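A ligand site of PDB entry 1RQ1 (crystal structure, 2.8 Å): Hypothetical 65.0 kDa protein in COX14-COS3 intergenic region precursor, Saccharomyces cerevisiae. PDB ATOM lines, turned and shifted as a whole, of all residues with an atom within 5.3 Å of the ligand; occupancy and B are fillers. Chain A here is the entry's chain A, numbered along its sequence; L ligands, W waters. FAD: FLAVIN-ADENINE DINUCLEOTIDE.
NE2 of His 193 lies within hydrogen-bond range of O1A of the ligand, at 2.9 Å. N of Thr 151 sits at hydrogen-bond distance from O2 of the ligand (2.7 Å). A nitrogen (N1A) of the ligand is in hydrogen-bond range of the side-chain hydroxyl (OH) of Tyr 166 (3.2 Å). The indole nitrogen of Trp 162 sits at hydrogen-bond distance from an oxygen (O2') of the ligand, at 3.0 Å. O2B of the ligand sits at hydrogen-bond distance from NH2 of Arg 229, 3.1 Å away. A nitrogen (N1A) of the ligand lies within hydrogen-bond range of the side-chain hydroxyl of Ser 190, at 2.7 Å. A nitrogen (N6A) of the ligand lies within hydrogen-bond range of the backbone carbonyl oxygen (O) of Ser 190 (3.1 Å). The side-chain hydroxyl (OG1) of Thr 151 lies within hydrogen-bond range of an oxygen (O2) of the ligand, 3.5 Å away. The guanidinium group (NE) of Arg 222 is in salt-bridge range of an oxygen (O1P) of the ligand (3.4 Å). The backbone carbonyl oxygen of Arg 149 is in hydrogen-bond range of a nitrogen (N3) of the ligand, 2.9 Å away. The side-chain carboxylate (OD2) of Asp 70 sits close to an oxygen (O4') of the ligand (3.4 Å).
The side-chain sulfur (SG) of Cys 317 is in hydrogen-bond range of the side-chain hydroxyl (OG1) of Thr 151, 3.6 Å away. N of Asp 70 sits at hydrogen-bond distance from O of Gly 152. NE2 of His 193 is in hydrogen-bond range of NE1 of Trp 162, 3.4 Å away. A ring nitrogen (ND1) of His 193 sits at hydrogen-bond distance from the side-chain hydroxyl (OH) of Tyr 166 (2.7 Å). The backbone carbonyl oxygen (O) of Arg 222 lies within hydrogen-bond range of the guanidinium group (NH1) of Arg 229. OG of Ser 190 is in hydrogen-bond range of OD1 of Asn 232 (2.8 Å). The side-chain hydroxyl (OG1) of Thr 151 sits at hydrogen-bond distance from the backbone NH (N) of Tyr 153, 3.2 Å away. The guanidinium group of Arg 222 is in salt-bridge range of the side-chain carboxylate of Asp 70 (2.7 Å).
A nitrogen (N5) of the ligand lies close to the side-chain sulfur (SG) of Cys 317 (3.7 Å). CG of Glu 148 touches O4 of the ligand, at 3.5 Å. Phe 150 touches the ligand (CA to O2, 3.5 Å). Gly 152 touches the ligand. CE2 of Tyr 153 touches C9 of the ligand, 3.6 Å away. Gly 154 touches the ligand. CB of Ala 158 touches O3' of the ligand (3.4 Å). Ile 161 touches the ligand (CG2 to C8M, 3.5 Å). OH of Tyr 186 touches C2A of the ligand, 3.5 Å away. Ala 194 touches the ligand (N to N6A, 3.6 Å). Ile 196 touches the ligand (CG2 to C4X, 3.5 Å). Leu 200 touches the ligand (CD2 to O4', 3.5 Å). Met 309 touches the ligand (CE to C7M, 3.2 Å). Hydrophobic or aromatic side chains that line the ligand: Phe 150, Tyr 153, Ala 158, Ile 161, Trp 162, Tyr 166, His 193, Ala 194, Ile 196, Leu 200 and Met 309.
Water W2 lies within hydrogen-bond range of an oxygen (O2') of the ligand (2.8 Å) and the backbone carbonyl oxygen (O) of His 193 (2.8 Å).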
ATOM      1  N   ASP A  70     -10.167  41.190 -23.929  1.00  0.00           N
ATOM      2  CA  ASP A  70     -10.505  40.818 -22.557  1.00  0.00           C
ATOM      3  C   ASP A  70     -10.247  42.027 -21.654  1.00  0.00           C
ATOM      4  O   ASP A  70      -9.270  42.753 -21.829  1.00  0.00           O
ATOM      5  CB  ASP A  70      -9.641  39.643 -22.102  1.00  0.00           C
ATOM      6  CG  ASP A  70     -10.175  38.992 -20.848  1.00  0.00           C
ATOM      7  OD1 ASP A  70     -10.964  39.640 -20.120  1.00  0.00           O
ATOM      8  OD2 ASP A  70      -9.806  37.823 -20.569  1.00  0.00           O
ATOM      9  N   GLU A 148       0.373  28.296 -27.984  1.00  0.00           N
ATOM     10  CA  GLU A 148      -0.898  28.806 -27.515  1.00  0.00           C
ATOM     11  C   GLU A 148      -0.552  29.492 -26.198  1.00  0.00           C
ATOM     12  O   GLU A 148       0.212  28.947 -25.394  1.00  0.00           O
ATOM     13  CB  GLU A 148      -1.879  27.650 -27.281  1.00  0.00           C
ATOM     14  CG  GLU A 148      -3.240  28.052 -26.787  1.00  0.00           C
ATOM     15  CD  GLU A 148      -4.152  26.875 -26.592  1.00  0.00           C
ATOM     16  OE1 GLU A 148      -3.844  26.023 -25.741  1.00  0.00           O
ATOM     17  OE2 GLU A 148      -5.180  26.795 -27.301  1.00  0.00           O
ATOM     18  N   ARG A 149      -1.081  30.690 -25.976  1.00  0.00           N
ATOM     19  CA  ARG A 149      -0.800  31.427 -24.745  1.00  0.00           C
ATOM     20  C   ARG A 149      -1.729  32.618 -24.628  1.00  0.00           C
ATOM     21  O   ARG A 149      -2.542  32.854 -25.509  1.00  0.00           O
ATOM     22  CB  ARG A 149       0.678  31.871 -24.732  1.00  0.00           C
ATOM     23  CG  ARG A 149       1.147  32.711 -25.936  1.00  0.00           C
ATOM     24  CD  ARG A 149       1.008  34.201 -25.657  1.00  0.00           C
ATOM     25  NE  ARG A 149       1.291  35.064 -26.814  1.00  0.00           N
ATOM     26  CZ  ARG A 149       2.453  35.109 -27.456  1.00  0.00           C
ATOM     27  NH1 ARG A 149       3.470  34.341 -27.066  1.00  0.00           N
ATOM     28  NH2 ARG A 149       2.617  35.936 -28.478  1.00  0.00           N
ATOM     29  N   PHE A 150      -1.640  33.361 -23.534  1.00  0.00           N
ATOM     30  CA  PHE A 150      -2.490  34.522 -23.332  1.00  0.00           C
ATOM     31  C   PHE A 150      -2.301  35.530 -24.493  1.00  0.00           C
ATOM     32  O   PHE A 150      -1.174  35.899 -24.806  1.00  0.00           O
ATOM     33  CB  PHE A 150      -2.136  35.194 -21.993  1.00  0.00           C
ATOM     34  CG  PHE A 150      -2.863  36.481 -21.747  1.00  0.00           C
ATOM     35  CD1 PHE A 150      -4.236  36.493 -21.520  1.00  0.00           C
ATOM     36  CD2 PHE A 150      -2.164  37.702 -21.738  1.00  0.00           C
ATOM     37  CE1 PHE A 150      -4.930  37.700 -21.302  1.00  0.00           C
ATOM     38  CE2 PHE A 150      -2.827  38.908 -21.523  1.00  0.00           C
ATOM     39  CZ  PHE A 150      -4.222  38.919 -21.297  1.00  0.00           C
ATOM     40  N   THR A 151      -3.397  35.957 -25.120  1.00  0.00           N
ATOM     41  CA  THR A 151      -3.277  36.917 -26.225  1.00  0.00           C
ATOM     42  C   THR A 151      -4.054  38.188 -25.962  1.00  0.00           C
ATOM     43  O   THR A 151      -3.820  39.198 -26.599  1.00  0.00           O
ATOM     44  CB  THR A 151      -3.774  36.332 -27.588  1.00  0.00           C
ATOM     45  OG1 THR A 151      -5.209  36.366 -27.632  1.00  0.00           O
ATOM     46  CG2 THR A 151      -3.307  34.899 -27.763  1.00  0.00           C
ATOM     47  N   GLY A 152      -4.993  38.140 -25.015  1.00  0.00           N
ATOM     48  CA  GLY A 152      -5.789  39.306 -24.716  1.00  0.00           C
ATOM     49  C   GLY A 152      -7.125  39.313 -25.449  1.00  0.00           C
ATOM     50  O   GLY A 152      -7.899  40.287 -25.371  1.00  0.00           O
ATOM     51  N   TYR A 153      -7.394  38.240 -26.189  1.00  0.00           N
ATOM     52  CA  TYR A 153      -8.625  38.078 -26.938  1.00  0.00           C
ATOM     53  C   TYR A 153      -9.729  37.718 -25.957  1.00  0.00           C
ATOM     54  O   TYR A 153      -9.477  37.075 -24.941  1.00  0.00           O
ATOM     55  CB  TYR A 153      -8.436  36.947 -27.972  1.00  0.00           C
ATOM     56  CG  TYR A 153      -9.659  36.611 -28.828  1.00  0.00           C
ATOM     57  CD1 TYR A 153     -10.260  37.572 -29.624  1.00  0.00           C
ATOM     58  CD2 TYR A 153     -10.155  35.317 -28.879  1.00  0.00           C
ATOM     59  CE1 TYR A 153     -11.327  37.252 -30.457  1.00  0.00           C
ATOM     60  CE2 TYR A 153     -11.227  34.981 -29.693  1.00  0.00           C
ATOM     61  CZ  TYR A 153     -11.806  35.952 -30.492  1.00  0.00           C
ATOM     62  OH  TYR A 153     -12.836  35.618 -31.337  1.00  0.00           O
ATOM     63  N   GLY A 154     -10.949  38.153 -26.243  1.00  0.00           N
ATOM     64  CA  GLY A 154     -12.072  37.858 -25.372  1.00  0.00           C
ATOM     65  C   GLY A 154     -13.256  38.740 -25.724  1.00  0.00           C
ATOM     66  O   GLY A 154     -13.643  38.836 -26.896  1.00  0.00           O
ATOM     67  N   GLY A 155     -13.839  39.386 -24.729  1.00  0.00           N
ATOM     68  CA  GLY A 155     -14.968  40.264 -24.981  1.00  0.00           C
ATOM     69  C   GLY A 155     -16.189  39.572 -25.540  1.00  0.00           C
ATOM     70  O   GLY A 155     -16.332  38.343 -25.458  1.00  0.00           O
ATOM     71  N   ALA A 158     -15.468  36.738 -28.563  1.00  0.00           N
ATOM     72  CA  ALA A 158     -15.078  35.418 -28.073  1.00  0.00           C
ATOM     73  C   ALA A 158     -16.304  34.797 -27.420  1.00  0.00           C
ATOM     74  O   ALA A 158     -16.551  33.584 -27.553  1.00  0.00           O
ATOM     75  CB  ALA A 158     -13.949  35.569 -27.055  1.00  0.00           C
ATOM     76  N   GLY A 159     -17.083  35.628 -26.745  1.00  0.00           N
ATOM     77  CA  GLY A 159     -18.284  35.166 -26.077  1.00  0.00           C
ATOM     78  C   GLY A 159     -19.313  34.674 -27.052  1.00  0.00           C
ATOM     79  O   GLY A 159     -19.927  33.635 -26.842  1.00  0.00           O
ATOM     80  N   ILE A 161     -18.807  33.464 -29.955  1.00  0.00           N
ATOM     81  CA  ILE A 161     -18.341  32.229 -30.558  1.00  0.00           C
ATOM     82  C   ILE A 161     -18.521  31.012 -29.642  1.00  0.00           C
ATOM     83  O   ILE A 161     -19.100  30.014 -30.062  1.00  0.00           O
ATOM     84  CB  ILE A 161     -16.868  32.387 -31.002  1.00  0.00           C
ATOM     85  CG1 ILE A 161     -16.829  33.448 -32.117  1.00  0.00           C
ATOM     86  CG2 ILE A 161     -16.295  31.046 -31.457  1.00  0.00           C
ATOM     87  CD1 ILE A 161     -15.459  33.823 -32.603  1.00  0.00           C
ATOM     88  N   TRP A 162     -18.048  31.100 -28.400  1.00  0.00           N
ATOM     89  CA  TRP A 162     -18.206  29.982 -27.463  1.00  0.00           C
ATOM     90  C   TRP A 162     -19.692  29.717 -27.269  1.00  0.00           C
ATOM     91  O   TRP A 162     -20.144  28.581 -27.189  1.00  0.00           O
ATOM     92  CB  TRP A 162     -17.587  30.317 -26.105  1.00  0.00           C
ATOM     93  CG  TRP A 162     -16.114  30.206 -26.080  1.00  0.00           C
ATOM     94  CD1 TRP A 162     -15.226  31.196 -25.805  1.00  0.00           C
ATOM     95  CD2 TRP A 162     -15.335  29.017 -26.309  1.00  0.00           C
ATOM     96  NE1 TRP A 162     -13.933  30.709 -25.836  1.00  0.00           N
ATOM     97  CE2 TRP A 162     -13.977  29.376 -26.148  1.00  0.00           C
ATOM     98  CE3 TRP A 162     -15.656  27.702 -26.631  1.00  0.00           C
ATOM     99  CZ2 TRP A 162     -12.942  28.456 -26.295  1.00  0.00           C
ATOM    100  CZ3 TRP A 162     -14.625  26.780 -26.787  1.00  0.00           C
ATOM    101  CH2 TRP A 162     -13.282  27.172 -26.617  1.00  0.00           C
ATOM    102  N   ILE A 165     -21.163  27.725 -30.178  1.00  0.00           N
ATOM    103  CA  ILE A 165     -20.762  26.312 -30.158  1.00  0.00           C
ATOM    104  C   ILE A 165     -21.608  25.509 -29.171  1.00  0.00           C
ATOM    105  O   ILE A 165     -22.078  24.426 -29.518  1.00  0.00           O
ATOM    106  CB  ILE A 165     -19.275  26.134 -29.759  1.00  0.00           C
ATOM    107  CG1 ILE A 165     -18.349  26.778 -30.798  1.00  0.00           C
ATOM    108  CG2 ILE A 165     -18.952  24.648 -29.625  1.00  0.00           C
ATOM    109  CD1 ILE A 165     -16.884  26.701 -30.449  1.00  0.00           C
ATOM    110  N   TYR A 166     -21.777  26.027 -27.953  1.00  0.00           N
ATOM    111  CA  TYR A 166     -22.573  25.362 -26.912  1.00  0.00           C
ATOM    112  C   TYR A 166     -24.054  25.293 -27.306  1.00  0.00           C
ATOM    113  O   TYR A 166     -24.733  24.317 -27.013  1.00  0.00           O
ATOM    114  CB  TYR A 166     -22.483  26.108 -25.569  1.00  0.00           C
ATOM    115  CG  TYR A 166     -21.169  25.969 -24.825  1.00  0.00           C
ATOM    116  CD1 TYR A 166     -20.303  27.044 -24.699  1.00  0.00           C
ATOM    117  CD2 TYR A 166     -20.806  24.761 -24.226  1.00  0.00           C
ATOM    118  CE1 TYR A 166     -19.104  26.926 -23.997  1.00  0.00           C
ATOM    119  CE2 TYR A 166     -19.616  24.634 -23.518  1.00  0.00           C
ATOM    120  CZ  TYR A 166     -18.767  25.715 -23.407  1.00  0.00           C
ATOM    121  OH  TYR A 166     -17.585  25.593 -22.719  1.00  0.00           O
ATOM    122  N   TYR A 186     -21.282  18.435 -25.164  1.00  0.00           N
ATOM    123  CA  TYR A 186     -21.091  19.537 -24.236  1.00  0.00           C
ATOM    124  C   TYR A 186     -19.773  19.352 -23.470  1.00  0.00           C
ATOM    125  O   TYR A 186     -18.949  20.260 -23.393  1.00  0.00           O
ATOM    126  CB  TYR A 186     -22.261  19.614 -23.246  1.00  0.00           C
ATOM    127  CG  TYR A 186     -21.961  20.475 -22.056  1.00  0.00           C
ATOM    128  CD1 TYR A 186     -21.903  21.870 -22.176  1.00  0.00           C
ATOM    129  CD2 TYR A 186     -21.587  19.906 -20.833  1.00  0.00           C
ATOM    130  CE1 TYR A 186     -21.460  22.665 -21.116  1.00  0.00           C
ATOM    131  CE2 TYR A 186     -21.139  20.688 -19.784  1.00  0.00           C
ATOM    132  CZ  TYR A 186     -21.071  22.067 -19.927  1.00  0.00           C
ATOM    133  OH  TYR A 186     -20.577  22.834 -18.894  1.00  0.00           O
ATOM    134  N   SER A 190     -16.592  21.769 -23.371  1.00  0.00           N
ATOM    135  CA  SER A 190     -16.253  22.343 -22.090  1.00  0.00           C
ATOM    136  C   SER A 190     -14.781  22.067 -21.749  1.00  0.00           C
ATOM    137  O   SER A 190     -14.074  22.949 -21.258  1.00  0.00           O
ATOM    138  CB  SER A 190     -17.180  21.774 -21.001  1.00  0.00           C
ATOM    139  OG  SER A 190     -16.935  22.355 -19.734  1.00  0.00           O
ATOM    140  N   GLY A 191     -14.326  20.853 -22.033  1.00  0.00           N
ATOM    141  CA  GLY A 191     -12.928  20.517 -21.767  1.00  0.00           C
ATOM    142  C   GLY A 191     -11.985  21.288 -22.677  1.00  0.00           C
ATOM    143  O   GLY A 191     -10.873  21.649 -22.276  1.00  0.00           O
ATOM    144  N   PHE A 192     -12.429  21.531 -23.918  1.00  0.00           N
ATOM    145  CA  PHE A 192     -11.631  22.264 -24.898  1.00  0.00           C
ATOM    146  C   PHE A 192     -11.509  23.701 -24.388  1.00  0.00           C
ATOM    147  O   PHE A 192     -10.413  24.266 -24.350  1.00  0.00           O
ATOM    148  CB  PHE A 192     -12.332  22.205 -26.267  1.00  0.00           C
ATOM    149  CG  PHE A 192     -11.812  23.185 -27.293  1.00  0.00           C
ATOM    150  CD1 PHE A 192     -10.449  23.433 -27.436  1.00  0.00           C
ATOM    151  CD2 PHE A 192     -12.705  23.852 -28.148  1.00  0.00           C
ATOM    152  CE1 PHE A 192      -9.966  24.326 -28.400  1.00  0.00           C
ATOM    153  CE2 PHE A 192     -12.240  24.751 -29.127  1.00  0.00           C
ATOM    154  CZ  PHE A 192     -10.868  24.985 -29.247  1.00  0.00           C
ATOM    155  N   HIS A 193     -12.653  24.263 -23.993  1.00  0.00           N
ATOM    156  CA  HIS A 193     -12.773  25.623 -23.462  1.00  0.00           C
ATOM    157  C   HIS A 193     -11.857  25.808 -22.238  1.00  0.00           C
ATOM    158  O   HIS A 193     -11.064  26.765 -22.171  1.00  0.00           O
ATOM    159  CB  HIS A 193     -14.237  25.858 -23.056  1.00  0.00           C
ATOM    160  CG  HIS A 193     -14.614  27.305 -22.904  1.00  0.00           C
ATOM    161  ND1 HIS A 193     -15.921  27.715 -22.812  1.00  0.00           N
ATOM    162  CD2 HIS A 193     -13.856  28.425 -22.886  1.00  0.00           C
ATOM    163  CE1 HIS A 193     -15.959  29.039 -22.732  1.00  0.00           C
ATOM    164  NE2 HIS A 193     -14.725  29.490 -22.775  1.00  0.00           N
ATOM    165  N   ALA A 194     -11.982  24.892 -21.280  1.00  0.00           N
ATOM    166  CA  ALA A 194     -11.208  24.936 -20.043  1.00  0.00           C
ATOM    167  C   ALA A 194      -9.717  24.798 -20.316  1.00  0.00           C
ATOM    168  O   ALA A 194      -8.907  25.437 -19.651  1.00  0.00           O
ATOM    169  CB  ALA A 194     -11.676  23.824 -19.086  1.00  0.00           C
ATOM    170  N   ILE A 196      -8.085  25.822 -22.893  1.00  0.00           N
ATOM    171  CA  ILE A 196      -7.567  27.079 -23.377  1.00  0.00           C
ATOM    172  C   ILE A 196      -7.446  28.054 -22.223  1.00  0.00           C
ATOM    173  O   ILE A 196      -6.417  28.704 -22.062  1.00  0.00           O
ATOM    174  CB  ILE A 196      -8.492  27.676 -24.459  1.00  0.00           C
ATOM    175  CG1 ILE A 196      -8.383  26.816 -25.719  1.00  0.00           C
ATOM    176  CG2 ILE A 196      -8.129  29.119 -24.748  1.00  0.00           C
ATOM    177  CD1 ILE A 196      -9.280  27.273 -26.824  1.00  0.00           C
ATOM    178  N   LEU A 200      -3.975  29.988 -21.168  1.00  0.00           N
ATOM    179  CA  LEU A 200      -3.708  31.416 -21.123  1.00  0.00           C
ATOM    180  C   LEU A 200      -3.382  31.826 -19.678  1.00  0.00           C
ATOM    181  O   LEU A 200      -2.761  32.867 -19.450  1.00  0.00           O
ATOM    182  CB  LEU A 200      -4.903  32.205 -21.673  1.00  0.00           C
ATOM    183  CG  LEU A 200      -6.281  32.101 -20.981  1.00  0.00           C
ATOM    184  CD1 LEU A 200      -6.313  33.041 -19.767  1.00  0.00           C
ATOM    185  CD2 LEU A 200      -7.386  32.489 -21.991  1.00  0.00           C
ATOM    186  N   ARG A 222     -11.124  31.313 -13.769  1.00  0.00           N
ATOM    187  CA  ARG A 222     -11.626  30.646 -14.972  1.00  0.00           C
ATOM    188  C   ARG A 222     -11.841  29.134 -14.826  1.00  0.00           C
ATOM    189  O   ARG A 222     -12.851  28.598 -15.299  1.00  0.00           O
ATOM    190  CB  ARG A 222     -10.671  30.895 -16.138  1.00  0.00           C
ATOM    191  CG  ARG A 222     -10.384  32.368 -16.432  1.00  0.00           C
ATOM    192  CD  ARG A 222     -11.658  33.143 -16.759  1.00  0.00           C
ATOM    193  NE  ARG A 222     -11.384  34.520 -17.182  1.00  0.00           N
ATOM    194  CZ  ARG A 222     -10.723  34.848 -18.286  1.00  0.00           C
ATOM    195  NH1 ARG A 222     -10.274  33.898 -19.103  1.00  0.00           N
ATOM    196  NH2 ARG A 222     -10.515  36.125 -18.582  1.00  0.00           N
ATOM    197  N   ASP A 228     -16.182  21.104 -12.257  1.00  0.00           N
ATOM    198  CA  ASP A 228     -16.679  20.502 -13.490  1.00  0.00           C
ATOM    199  C   ASP A 228     -15.755  20.804 -14.690  1.00  0.00           C
ATOM    200  O   ASP A 228     -15.560  19.954 -15.561  1.00  0.00           O
ATOM    201  CB  ASP A 228     -18.114  21.013 -13.763  1.00  0.00           C
ATOM    202  CG  ASP A 228     -18.165  22.526 -13.987  1.00  0.00           C
ATOM    203  OD1 ASP A 228     -17.666  23.282 -13.113  1.00  0.00           O
ATOM    204  OD2 ASP A 228     -18.701  22.963 -15.041  1.00  0.00           O
ATOM    205  N   ARG A 229     -15.188  22.003 -14.727  1.00  0.00           N
ATOM    206  CA  ARG A 229     -14.313  22.387 -15.811  1.00  0.00           C
ATOM    207  C   ARG A 229     -12.986  21.640 -15.767  1.00  0.00           C
ATOM    208  O   ARG A 229     -12.417  21.314 -16.804  1.00  0.00           O
ATOM    209  CB  ARG A 229     -14.064  23.895 -15.778  1.00  0.00           C
ATOM    210  CG  ARG A 229     -15.308  24.700 -16.070  1.00  0.00           C
ATOM    211  CD  ARG A 229     -15.066  26.189 -15.949  1.00  0.00           C
ATOM    212  NE  ARG A 229     -16.329  26.923 -16.043  1.00  0.00           N
ATOM    213  CZ  ARG A 229     -16.438  28.250 -15.952  1.00  0.00           C
ATOM    214  NH1 ARG A 229     -15.348  28.987 -15.775  1.00  0.00           N
ATOM    215  NH2 ARG A 229     -17.629  28.824 -16.061  1.00  0.00           N
ATOM    216  N   ASN A 232     -13.721  18.051 -16.958  1.00  0.00           N
ATOM    217  CA  ASN A 232     -13.892  17.974 -18.392  1.00  0.00           C
ATOM    218  C   ASN A 232     -12.574  17.916 -19.150  1.00  0.00           C
ATOM    219  O   ASN A 232     -12.486  17.308 -20.203  1.00  0.00           O
ATOM    220  CB  ASN A 232     -14.774  19.126 -18.855  1.00  0.00           C
ATOM    221  CG  ASN A 232     -16.249  18.929 -18.480  1.00  0.00           C
ATOM    222  OD1 ASN A 232     -17.061  19.848 -18.574  1.00  0.00           O
ATOM    223  ND2 ASN A 232     -16.591  17.718 -18.057  1.00  0.00           N
ATOM    224  N   MET A 309     -14.270  28.343 -36.168  1.00  0.00           N
ATOM    225  CA  MET A 309     -12.928  28.758 -35.832  1.00  0.00           C
ATOM    226  C   MET A 309     -12.469  29.877 -36.763  1.00  0.00           C
ATOM    227  O   MET A 309     -11.650  30.720 -36.383  1.00  0.00           O
ATOM    228  CB  MET A 309     -11.961  27.582 -35.892  1.00  0.00           C
ATOM    229  CG  MET A 309     -12.270  26.465 -34.873  1.00  0.00           C
ATOM    230  SD  MET A 309     -12.589  27.059 -33.171  1.00  0.00           S
ATOM    231  CE  MET A 309     -11.164  28.080 -33.011  1.00  0.00           C
ATOM    232  N   VAL A 312     -12.907  33.395 -35.544  1.00  0.00           N
ATOM    233  CA  VAL A 312     -12.010  33.837 -34.481  1.00  0.00           C
ATOM    234  C   VAL A 312     -11.012  34.831 -35.056  1.00  0.00           C
ATOM    235  O   VAL A 312     -10.126  34.455 -35.809  1.00  0.00           O
ATOM    236  CB  VAL A 312     -11.266  32.625 -33.891  1.00  0.00           C
ATOM    237  CG1 VAL A 312     -10.224  33.066 -32.875  1.00  0.00           C
ATOM    238  CG2 VAL A 312     -12.284  31.680 -33.252  1.00  0.00           C
ATOM    239  N   ARG A 316      -3.614  33.563 -33.512  1.00  0.00           N
ATOM    240  CA  ARG A 316      -3.068  32.408 -32.786  1.00  0.00           C
ATOM    241  C   ARG A 316      -4.179  31.572 -32.165  1.00  0.00           C
ATOM    242  O   ARG A 316      -4.034  30.362 -32.008  1.00  0.00           O
ATOM    243  CB  ARG A 316      -2.095  32.856 -31.704  1.00  0.00           C
ATOM    244  CG  ARG A 316      -0.781  33.300 -32.284  1.00  0.00           C
ATOM    245  CD  ARG A 316       0.107  33.913 -31.239  1.00  0.00           C
ATOM    246  NE  ARG A 316       1.009  32.950 -30.608  1.00  0.00           N
ATOM    247  CZ  ARG A 316       2.323  33.107 -30.589  1.00  0.00           C
ATOM    248  NH1 ARG A 316       2.869  34.169 -31.183  1.00  0.00           N
ATOM    249  NH2 ARG A 316       3.095  32.238 -29.954  1.00  0.00           N
ATOM    250  N   CYS A 317      -5.274  32.228 -31.806  1.00  0.00           N
ATOM    251  CA  CYS A 317      -6.394  31.537 -31.219  1.00  0.00           C
ATOM    252  C   CYS A 317      -7.069  30.717 -32.299  1.00  0.00           C
ATOM    253  O   CYS A 317      -7.519  29.606 -32.046  1.00  0.00           O
ATOM    254  CB  CYS A 317      -7.407  32.523 -30.667  1.00  0.00           C
ATOM    255  SG  CYS A 317      -6.758  33.822 -29.575  1.00  0.00           S
ATOM    256  N   GLY A 321      -7.211  26.813 -32.165  1.00  0.00           N
ATOM    257  CA  GLY A 321      -8.595  26.402 -32.049  1.00  0.00           C
ATOM    258  C   GLY A 321      -8.876  25.375 -33.126  1.00  0.00           C
ATOM    259  O   GLY A 321      -9.432  24.305 -32.877  1.00  0.00           O
HETATM  260  PA  FAD L   1     -14.992  32.740 -20.998  1.00  0.00           P
HETATM  261  O1A FAD L   1     -14.865  32.329 -22.440  1.00  0.00           O
HETATM  262  O2A FAD L   1     -14.175  32.390 -19.804  1.00  0.00           O
HETATM  263  O5B FAD L   1     -16.567  32.808 -20.872  1.00  0.00           O
HETATM  264  C5B FAD L   1     -17.599  32.171 -21.614  1.00  0.00           C
HETATM  265  C4B FAD L   1     -18.721  31.857 -20.659  1.00  0.00           C
HETATM  266  O4B FAD L   1     -18.817  30.406 -20.711  1.00  0.00           O
HETATM  267  C3B FAD L   1     -18.897  32.315 -19.194  1.00  0.00           C
HETATM  268  O3B FAD L   1     -20.290  32.630 -19.071  1.00  0.00           O
HETATM  269  C2B FAD L   1     -18.485  31.136 -18.444  1.00  0.00           C
HETATM  270  O2B FAD L   1     -19.392  31.064 -17.392  1.00  0.00           O
HETATM  271  C1B FAD L   1     -18.513  29.923 -19.398  1.00  0.00           C
HETATM  272  N9A FAD L   1     -17.340  29.120 -19.414  1.00  0.00           N
HETATM  273  C8A FAD L   1     -15.954  29.397 -19.291  1.00  0.00           C
HETATM  274  N7A FAD L   1     -15.241  28.303 -19.274  1.00  0.00           N
HETATM  275  C5A FAD L   1     -16.144  27.242 -19.387  1.00  0.00           C
HETATM  276  C6A FAD L   1     -16.120  25.829 -19.449  1.00  0.00           C
HETATM  277  N6A FAD L   1     -14.921  25.260 -19.323  1.00  0.00           N
HETATM  278  N1A FAD L   1     -17.220  25.007 -19.600  1.00  0.00           N
HETATM  279  C2A FAD L   1     -18.465  25.535 -19.648  1.00  0.00           C
HETATM  280  N3A FAD L   1     -18.520  26.943 -19.604  1.00  0.00           N
HETATM  281  C4A FAD L   1     -17.357  27.729 -19.474  1.00  0.00           C
HETATM  282  N1  FAD L   1      -7.429  33.479 -25.460  1.00  0.00           N
HETATM  283  C2  FAD L   1      -6.072  33.655 -25.251  1.00  0.00           C
HETATM  284  O2  FAD L   1      -5.736  34.702 -24.649  1.00  0.00           O
HETATM  285  N3  FAD L   1      -5.417  32.656 -25.937  1.00  0.00           N
HETATM  286  C4  FAD L   1      -5.978  31.658 -26.785  1.00  0.00           C
HETATM  287  O4  FAD L   1      -5.060  30.977 -27.361  1.00  0.00           O
HETATM  288  C4X FAD L   1      -7.344  31.644 -27.010  1.00  0.00           C
HETATM  289  N5  FAD L   1      -8.065  30.822 -27.943  1.00  0.00           N
HETATM  290  C5X FAD L   1      -9.471  30.814 -28.184  1.00  0.00           C
HETATM  291  C6  FAD L   1     -10.072  29.867 -29.038  1.00  0.00           C
HETATM  292  C7  FAD L   1     -11.459  29.992 -29.323  1.00  0.00           C
HETATM  293  C7M FAD L   1     -12.068  28.798 -30.052  1.00  0.00           C
HETATM  294  C8  FAD L   1     -12.279  31.036 -28.821  1.00  0.00           C
HETATM  295  C8M FAD L   1     -13.756  31.263 -29.113  1.00  0.00           C
HETATM  296  C9  FAD L   1     -11.647  31.920 -27.931  1.00  0.00           C
HETATM  297  C9A FAD L   1     -10.300  31.843 -27.503  1.00  0.00           C
HETATM  298  N10 FAD L   1      -9.488  32.574 -26.487  1.00  0.00           N
HETATM  299  C10 FAD L   1      -8.122  32.588 -26.262  1.00  0.00           C
HETATM  300  C1' FAD L   1     -10.233  33.448 -25.646  1.00  0.00           C
HETATM  301  C2' FAD L   1     -10.836  32.934 -24.384  1.00  0.00           C
HETATM  302  O2' FAD L   1     -11.437  31.614 -24.493  1.00  0.00           O
HETATM  303  C3' FAD L   1     -11.738  33.984 -23.822  1.00  0.00           C
HETATM  304  O3' FAD L   1     -13.119  34.036 -24.148  1.00  0.00           O
HETATM  305  C4' FAD L   1     -11.360  34.650 -22.504  1.00  0.00           C
HETATM  306  O4' FAD L   1     -10.023  34.761 -21.950  1.00  0.00           O
HETATM  307  C5' FAD L   1     -11.987  35.927 -22.177  1.00  0.00           C
HETATM  308  O5' FAD L   1     -12.665  35.171 -21.168  1.00  0.00           O
HETATM  309  P   FAD L   1     -14.018  35.605 -20.515  1.00  0.00           P
HETATM  310  O1P FAD L   1     -13.968  35.595 -19.058  1.00  0.00           O
HETATM  311  O2P FAD L   1     -14.588  36.850 -21.094  1.00  0.00           O
HETATM  312  O3P FAD L   1     -14.885  34.290 -20.727  1.00  0.00           O
HETATM  313  O   HOH W   1     -12.627  28.336 -19.044  1.00  0.00           O
HETATM  314  O   HOH W   2     -11.147  29.570 -22.593  1.00  0.00           O
